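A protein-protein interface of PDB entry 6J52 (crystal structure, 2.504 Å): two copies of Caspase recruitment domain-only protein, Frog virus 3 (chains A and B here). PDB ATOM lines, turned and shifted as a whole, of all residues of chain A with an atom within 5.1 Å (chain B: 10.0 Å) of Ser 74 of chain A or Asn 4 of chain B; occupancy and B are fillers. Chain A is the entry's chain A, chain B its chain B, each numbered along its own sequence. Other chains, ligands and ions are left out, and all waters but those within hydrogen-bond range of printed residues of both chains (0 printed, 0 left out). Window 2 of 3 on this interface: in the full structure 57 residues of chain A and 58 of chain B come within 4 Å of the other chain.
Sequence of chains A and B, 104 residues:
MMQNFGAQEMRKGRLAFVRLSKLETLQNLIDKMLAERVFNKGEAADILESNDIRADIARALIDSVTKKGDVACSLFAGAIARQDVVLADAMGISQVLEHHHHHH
The backbone NH of Ala 7 of chain B sits at hydrogen-bond distance from the side-chain carboxylate of Asp 70 of chain A (3.1 Å).
OG of Ser 74 of chain A lies close to O of Gln 3 of chain B (3.5 Å).
The side-chain hydroxyl (OG) of Ser 74 of chain A sits at hydrogen-bond distance from the backbone NH (N) of Phe 5 of chain B, at 3.0 Å.
O of Phe 5 of chain B sits close to O of Cys 73 of chain A (3.3 Å).
Among the printed residues, merely in contact across the chains: Cys 73 of chain A with Met 10 of chain B, Ala 77 of chain A with Phe 5 of chain B, Cys 73 of chain A with Ala 7 of chain B, Phe 76 of chain A with Met 33 of chain B, Phe 76 of chain A with Met 10 of chain B, Cys 73 of chain A with Gly 6 of chain B, Ser 74 of chain A with Asn 4 of chain B, Phe 76 of chain A with Leu 29 of chain B, Asp 70 of chain A with Gly 6 of chain B and Asp 70 of chain A with Phe 5 of chain B.
No position is printed for both chains.
Of the 14 pairs that touch across the chains among the printed residues, none has its exchanged pair printed and touching as well.
Of the printed residues of chain B, Asp 70 of chain A touches Phe 5, Gly 6 and Ala 7.
Ser 74 of chain A touches just these residues of chain B: Gln 3, Asn 4 and Phe 5.
Of chain B, only Phe 5 (3.5 Å) comes within 4 Å of Ala 77 of chain A.
Asn 4 of chain B touches just one residue of chain A: Ser 74.
Of the printed residues of chain A, Met 10 of chain B touches Cys 73 (3.4 Å) and Phe 76 (3.8 Å).
Of the printed residues of chain A, Met 33 of chain B touches Phe 76 (3.7 Å).
Glu 36 of chain B touches none of the printed residues of chain A.
The nearest residue of chain B that does not touch Ser 74 of chain A is Gly 6 of chain B (4.1 Å).
The nearest printed residue of chain A that does not touch Asn 4 of chain B is Asp 70 of chain A (5.8 Å).
The nearest printed residue of chain A that does not touch Leu 29 of chain B is Gly 78 of chain A (6.6 Å).
O of Gly 69 of chain A sits at hydrogen-bond distance from SG of Cys 73 of chain A (3.1 Å).
The backbone carbonyl oxygen (O) of Asp 70 of chain A sits at hydrogen-bond distance from the side-chain hydroxyl (OG) of Ser 74 of chain A (3.0 Å).
The backbone NH (N) of Gly 6 of chain B sits at hydrogen-bond distance from the side-chain carboxylate (OE2) of Glu 9 of chain B.
O of Met 33 of chain B is in hydrogen-bond range of N of Val 38 of chain B.
Of the 10 printed residues of chain A, 5 touch a printed residue of chain B.
Hydrophobic or aromatic side chains of chain A that line the printed part of chain B: Phe 76 and Ala 77.
Hydrophobic or aromatic side chains of chain B within 4 Å of the printed part of chain A: Phe 5, Ala 7, Met 10, Leu 29 and Met 33.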
ATOM      1  N   GLY A  69      31.116  22.328  10.394  1.00  0.00           N
ATOM      2  CA  GLY A  69      31.743  21.776   9.199  1.00  0.00           C
ATOM      3  C   GLY A  69      31.451  20.305   8.972  1.00  0.00           C
ATOM      4  O   GLY A  69      30.558  19.706   9.573  1.00  0.00           O
ATOM      5  N   ASP A  70      32.264  19.706   8.099  1.00  0.00           N
ATOM      6  CA  ASP A  70      31.901  18.419   7.514  1.00  0.00           C
ATOM      7  C   ASP A  70      32.053  17.265   8.497  1.00  0.00           C
ATOM      8  O   ASP A  70      31.215  16.352   8.511  1.00  0.00           O
ATOM      9  CB  ASP A  70      32.723  18.159   6.247  1.00  0.00           C
ATOM     10  CG  ASP A  70      32.498  19.224   5.160  1.00  0.00           C
ATOM     11  OD1 ASP A  70      31.498  19.975   5.230  1.00  0.00           O
ATOM     12  OD2 ASP A  70      33.335  19.314   4.229  1.00  0.00           O
ATOM     13  N   VAL A  71      33.099  17.285   9.331  1.00  0.00           N
ATOM     14  CA  VAL A  71      33.315  16.175  10.259  1.00  0.00           C
ATOM     15  C   VAL A  71      32.215  16.128  11.313  1.00  0.00           C
ATOM     16  O   VAL A  71      31.732  15.048  11.683  1.00  0.00           O
ATOM     17  CB  VAL A  71      34.709  16.270  10.901  1.00  0.00           C
ATOM     18  CG1 VAL A  71      34.878  15.187  11.958  1.00  0.00           C
ATOM     19  CG2 VAL A  71      35.772  16.127   9.842  1.00  0.00           C
ATOM     20  N   ALA A  72      31.810  17.289  11.825  1.00  0.00           N
ATOM     21  CA  ALA A  72      30.699  17.309  12.766  1.00  0.00           C
ATOM     22  C   ALA A  72      29.409  16.848  12.083  1.00  0.00           C
ATOM     23  O   ALA A  72      28.673  16.005  12.619  1.00  0.00           O
ATOM     24  CB  ALA A  72      30.554  18.706  13.362  1.00  0.00           C
ATOM     25  N   CYS A  73      29.130  17.377  10.885  1.00  0.00           N
ATOM     26  CA  CYS A  73      27.957  16.933  10.131  1.00  0.00           C
ATOM     27  C   CYS A  73      27.981  15.426   9.906  1.00  0.00           C
ATOM     28  O   CYS A  73      26.925  14.779   9.896  1.00  0.00           O
ATOM     29  CB  CYS A  73      27.863  17.663   8.792  1.00  0.00           C
ATOM     30  SG  CYS A  73      27.498  19.410   8.944  1.00  0.00           S
ATOM     31  N   SER A  74      29.169  14.838   9.729  1.00  0.00           N
ATOM     32  CA  SER A  74      29.197  13.405   9.466  1.00  0.00           C
ATOM     33  C   SER A  74      28.906  12.617  10.730  1.00  0.00           C
ATOM     34  O   SER A  74      28.198  11.605  10.686  1.00  0.00           O
ATOM     35  CB  SER A  74      30.525  12.992   8.850  1.00  0.00           C
ATOM     36  OG  SER A  74      30.639  13.536   7.551  1.00  0.00           O
ATOM     37  N   LEU A  75      29.409  13.082  11.872  1.00  0.00           N
ATOM     38  CA  LEU A  75      29.036  12.451  13.132  1.00  0.00           C
ATOM     39  C   LEU A  75      27.539  12.609  13.383  1.00  0.00           C
ATOM     40  O   LEU A  75      26.832  11.631  13.653  1.00  0.00           O
ATOM     41  CB  LEU A  75      29.877  13.033  14.274  1.00  0.00           C
ATOM     42  CG  LEU A  75      31.391  12.778  14.101  1.00  0.00           C
ATOM     43  CD1 LEU A  75      32.291  13.670  14.969  1.00  0.00           C
ATOM     44  CD2 LEU A  75      31.709  11.314  14.351  1.00  0.00           C
ATOM     45  N   PHE A  76      27.030  13.833  13.248  1.00  0.00           N
ATOM     46  CA  PHE A  76      25.593  14.056  13.350  1.00  0.00           C
ATOM     47  C   PHE A  76      24.791  13.092  12.463  1.00  0.00           C
ATOM     48  O   PHE A  76      23.791  12.518  12.909  1.00  0.00           O
ATOM     49  CB  PHE A  76      25.270  15.515  13.005  1.00  0.00           C
ATOM     50  CG  PHE A  76      23.908  15.956  13.473  1.00  0.00           C
ATOM     51  CD1 PHE A  76      23.565  15.868  14.815  1.00  0.00           C
ATOM     52  CD2 PHE A  76      22.959  16.429  12.570  1.00  0.00           C
ATOM     53  CE1 PHE A  76      22.300  16.259  15.258  1.00  0.00           C
ATOM     54  CE2 PHE A  76      21.690  16.826  13.003  1.00  0.00           C
ATOM     55  CZ  PHE A  76      21.363  16.742  14.354  1.00  0.00           C
ATOM     56  N   ALA A  77      25.210  12.893  11.208  1.00  0.00           N
ATOM     57  CA  ALA A  77      24.425  12.038  10.312  1.00  0.00           C
ATOM     58  C   ALA A  77      24.481  10.577  10.742  1.00  0.00           C
ATOM     59  O   ALA A  77      23.481   9.857  10.626  1.00  0.00           O
ATOM     60  CB  ALA A  77      24.899  12.175   8.867  1.00  0.00           C
ATOM     61  N   GLY A  78      25.640  10.120  11.239  1.00  0.00           N
ATOM     62  CA  GLY A  78      25.709   8.788  11.815  1.00  0.00           C
ATOM     63  C   GLY A  78      24.772   8.617  13.000  1.00  0.00           C
ATOM     64  O   GLY A  78      24.127   7.574  13.158  1.00  0.00           O
ATOM     65  N   MET B   2      31.311   5.138  10.484  1.00  0.00           N
ATOM     66  CA  MET B   2      31.453   6.500   9.988  1.00  0.00           C
ATOM     67  C   MET B   2      30.785   6.668   8.608  1.00  0.00           C
ATOM     68  O   MET B   2      30.807   5.775   7.761  1.00  0.00           O
ATOM     69  CB  MET B   2      32.942   6.887   9.943  1.00  0.00           C
ATOM     70  CG  MET B   2      33.260   8.319   9.478  1.00  0.00           C
ATOM     71  SD  MET B   2      32.854   9.617  10.671  1.00  0.00           S
ATOM     72  CE  MET B   2      33.875  10.986  10.123  1.00  0.00           C
ATOM     73  N   GLN B   3      30.152   7.820   8.427  1.00  0.00           N
ATOM     74  CA  GLN B   3      29.592   8.286   7.167  1.00  0.00           C
ATOM     75  C   GLN B   3      30.429   9.436   6.631  1.00  0.00           C
ATOM     76  O   GLN B   3      31.154  10.104   7.371  1.00  0.00           O
ATOM     77  CB  GLN B   3      28.159   8.792   7.351  1.00  0.00           C
ATOM     78  CG  GLN B   3      27.196   7.796   7.904  1.00  0.00           C
ATOM     79  CD  GLN B   3      26.034   7.575   6.974  1.00  0.00           C
ATOM     80  OE1 GLN B   3      26.150   7.748   5.759  1.00  0.00           O
ATOM     81  NE2 GLN B   3      24.912   7.167   7.534  1.00  0.00           N
ATOM     82  N   ASN B   4      30.312   9.678   5.340  1.00  0.00           N
ATOM     83  CA  ASN B   4      30.837  10.901   4.749  1.00  0.00           C
ATOM     84  C   ASN B   4      29.612  11.681   4.310  1.00  0.00           C
ATOM     85  O   ASN B   4      29.114  11.522   3.193  1.00  0.00           O
ATOM     86  CB  ASN B   4      31.794  10.654   3.597  1.00  0.00           C
ATOM     87  CG  ASN B   4      32.520  11.921   3.175  1.00  0.00           C
ATOM     88  OD1 ASN B   4      32.186  13.021   3.628  1.00  0.00           O
ATOM     89  ND2 ASN B   4      33.519  11.778   2.312  1.00  0.00           N
ATOM     90  N   PHE B   5      29.133  12.523   5.209  1.00  0.00           N
ATOM     91  CA  PHE B   5      27.893  13.281   5.032  1.00  0.00           C
ATOM     92  C   PHE B   5      28.182  14.685   5.553  1.00  0.00           C
ATOM     93  O   PHE B   5      27.983  14.954   6.740  1.00  0.00           O
ATOM     94  CB  PHE B   5      26.744  12.619   5.780  1.00  0.00           C
ATOM     95  CG  PHE B   5      25.384  13.154   5.417  1.00  0.00           C
ATOM     96  CD1 PHE B   5      24.633  12.556   4.408  1.00  0.00           C
ATOM     97  CD2 PHE B   5      24.842  14.238   6.100  1.00  0.00           C
ATOM     98  CE1 PHE B   5      23.368  13.035   4.076  1.00  0.00           C
ATOM     99  CE2 PHE B   5      23.580  14.723   5.768  1.00  0.00           C
ATOM    100  CZ  PHE B   5      22.842  14.118   4.754  1.00  0.00           C
ATOM    101  N   GLY B   6      28.648  15.560   4.657  1.00  0.00           N
ATOM    102  CA  GLY B   6      29.131  16.874   5.026  1.00  0.00           C
ATOM    103  C   GLY B   6      28.048  17.938   5.029  1.00  0.00           C
ATOM    104  O   GLY B   6      26.856  17.661   4.863  1.00  0.00           O
ATOM    105  N   ALA B   7      28.493  19.194   5.191  1.00  0.00           N
ATOM    106  CA  ALA B   7      27.580  20.312   5.434  1.00  0.00           C
ATOM    107  C   ALA B   7      26.627  20.535   4.264  1.00  0.00           C
ATOM    108  O   ALA B   7      25.433  20.792   4.468  1.00  0.00           O
ATOM    109  CB  ALA B   7      28.373  21.591   5.728  1.00  0.00           C
ATOM    110  N   GLN B   8      27.139  20.445   3.036  1.00  0.00           N
ATOM    111  CA  GLN B   8      26.310  20.608   1.842  1.00  0.00           C
ATOM    112  C   GLN B   8      25.111  19.667   1.868  1.00  0.00           C
ATOM    113  O   GLN B   8      23.955  20.109   1.815  1.00  0.00           O
ATOM    114  CB  GLN B   8      27.156  20.375   0.593  1.00  0.00           C
ATOM    115  CG  GLN B   8      26.456  20.752  -0.710  1.00  0.00           C
ATOM    116  CD  GLN B   8      27.363  20.570  -1.924  1.00  0.00           C
ATOM    117  OE1 GLN B   8      26.891  20.444  -3.056  1.00  0.00           O
ATOM    118  NE2 GLN B   8      28.671  20.553  -1.689  1.00  0.00           N
ATOM    119  N   GLU B   9      25.366  18.360   1.974  1.00  0.00           N
ATOM    120  CA  GLU B   9      24.262  17.409   2.077  1.00  0.00           C
ATOM    121  C   GLU B   9      23.371  17.729   3.280  1.00  0.00           C
ATOM    122  O   GLU B   9      22.139  17.665   3.182  1.00  0.00           O
ATOM    123  CB  GLU B   9      24.804  15.977   2.164  1.00  0.00           C
ATOM    124  CG  GLU B   9      25.867  15.629   1.127  1.00  0.00           C
ATOM    125  CD  GLU B   9      27.295  15.907   1.622  1.00  0.00           C
ATOM    126  OE1 GLU B   9      27.649  17.099   1.809  1.00  0.00           O
ATOM    127  OE2 GLU B   9      28.067  14.936   1.825  1.00  0.00           O
ATOM    128  N   MET B  10      23.982  18.093   4.417  1.00  0.00           N
ATOM    129  CA  MET B  10      23.208  18.389   5.616  1.00  0.00           C
ATOM    130  C   MET B  10      22.243  19.547   5.376  1.00  0.00           C
ATOM    131  O   MET B  10      21.094  19.511   5.836  1.00  0.00           O
ATOM    132  CB  MET B  10      24.145  18.691   6.787  1.00  0.00           C
ATOM    133  CG  MET B  10      23.446  18.877   8.131  1.00  0.00           C
ATOM    134  SD  MET B  10      22.619  17.367   8.666  1.00  0.00           S
ATOM    135  CE  MET B  10      24.011  16.280   8.969  1.00  0.00           C
ATOM    136  N   LEU B  29      19.824  13.355  20.176  1.00  0.00           N
ATOM    137  CA  LEU B  29      20.912  13.836  19.336  1.00  0.00           C
ATOM    138  C   LEU B  29      21.747  14.870  20.077  1.00  0.00           C
ATOM    139  O   LEU B  29      22.981  14.874  19.975  1.00  0.00           O
ATOM    140  CB  LEU B  29      20.345  14.404  18.035  1.00  0.00           C
ATOM    141  CG  LEU B  29      19.710  13.371  17.090  1.00  0.00           C
ATOM    142  CD1 LEU B  29      18.932  14.069  15.969  1.00  0.00           C
ATOM    143  CD2 LEU B  29      20.768  12.449  16.508  1.00  0.00           C
ATOM    144  N   LYS B  32      23.921  12.938  22.323  1.00  0.00           N
ATOM    145  CA  LYS B  32      24.969  12.282  21.555  1.00  0.00           C
ATOM    146  C   LYS B  32      26.052  13.279  21.132  1.00  0.00           C
ATOM    147  O   LYS B  32      27.249  13.009  21.286  1.00  0.00           O
ATOM    148  CB  LYS B  32      24.368  11.572  20.344  1.00  0.00           C
ATOM    149  CG  LYS B  32      25.424  10.898  19.479  1.00  0.00           C
ATOM    150  CD  LYS B  32      26.161   9.827  20.263  1.00  0.00           C
ATOM    151  CE  LYS B  32      27.044   8.998  19.356  1.00  0.00           C
ATOM    152  NZ  LYS B  32      27.842   7.995  20.119  1.00  0.00           N
ATOM    153  N   MET B  33      25.651  14.446  20.609  1.00  0.00           N
ATOM    154  CA  MET B  33      26.647  15.428  20.181  1.00  0.00           C
ATOM    155  C   MET B  33      27.453  15.972  21.360  1.00  0.00           C
ATOM    156  O   MET B  33      28.603  16.403  21.187  1.00  0.00           O
ATOM    157  CB  MET B  33      25.977  16.568  19.415  1.00  0.00           C
ATOM    158  CG  MET B  33      25.499  16.192  18.011  1.00  0.00           C
ATOM    159  SD  MET B  33      26.685  15.433  16.882  1.00  0.00           S
ATOM    160  CE  MET B  33      26.576  13.686  17.261  1.00  0.00           C
ATOM    161  N   GLU B  36      30.073  13.162  21.916  1.00  0.00           N
ATOM    162  CA  GLU B  36      31.119  13.163  20.906  1.00  0.00           C
ATOM    163  C   GLU B  36      32.013  14.401  20.960  1.00  0.00           C
ATOM    164  O   GLU B  36      32.864  14.565  20.074  1.00  0.00           O
ATOM    165  CB  GLU B  36      30.493  13.028  19.515  1.00  0.00           C
ATOM    166  CG  GLU B  36      29.722  11.733  19.313  1.00  0.00           C
ATOM    167  CD  GLU B  36      30.569  10.500  19.595  1.00  0.00           C
ATOM    168  OE1 GLU B  36      30.208   9.717  20.506  1.00  0.00           O
ATOM    169  OE2 GLU B  36      31.598  10.316  18.903  1.00  0.00           O
ATOM    170  N   VAL B  38      31.227  17.273  20.202  1.00  0.00           N
ATOM    171  CA  VAL B  38      30.843  18.245  19.188  1.00  0.00           C
ATOM    172  C   VAL B  38      30.331  19.515  19.851  1.00  0.00           C
ATOM    173  O   VAL B  38      30.627  20.635  19.407  1.00  0.00           O
ATOM    174  CB  VAL B  38      29.793  17.621  18.248  1.00  0.00           C
ATOM    175  CG1 VAL B  38      29.261  18.645  17.258  1.00  0.00           C
ATOM    176  CG2 VAL B  38      30.397  16.443  17.535  1.00  0.00           C
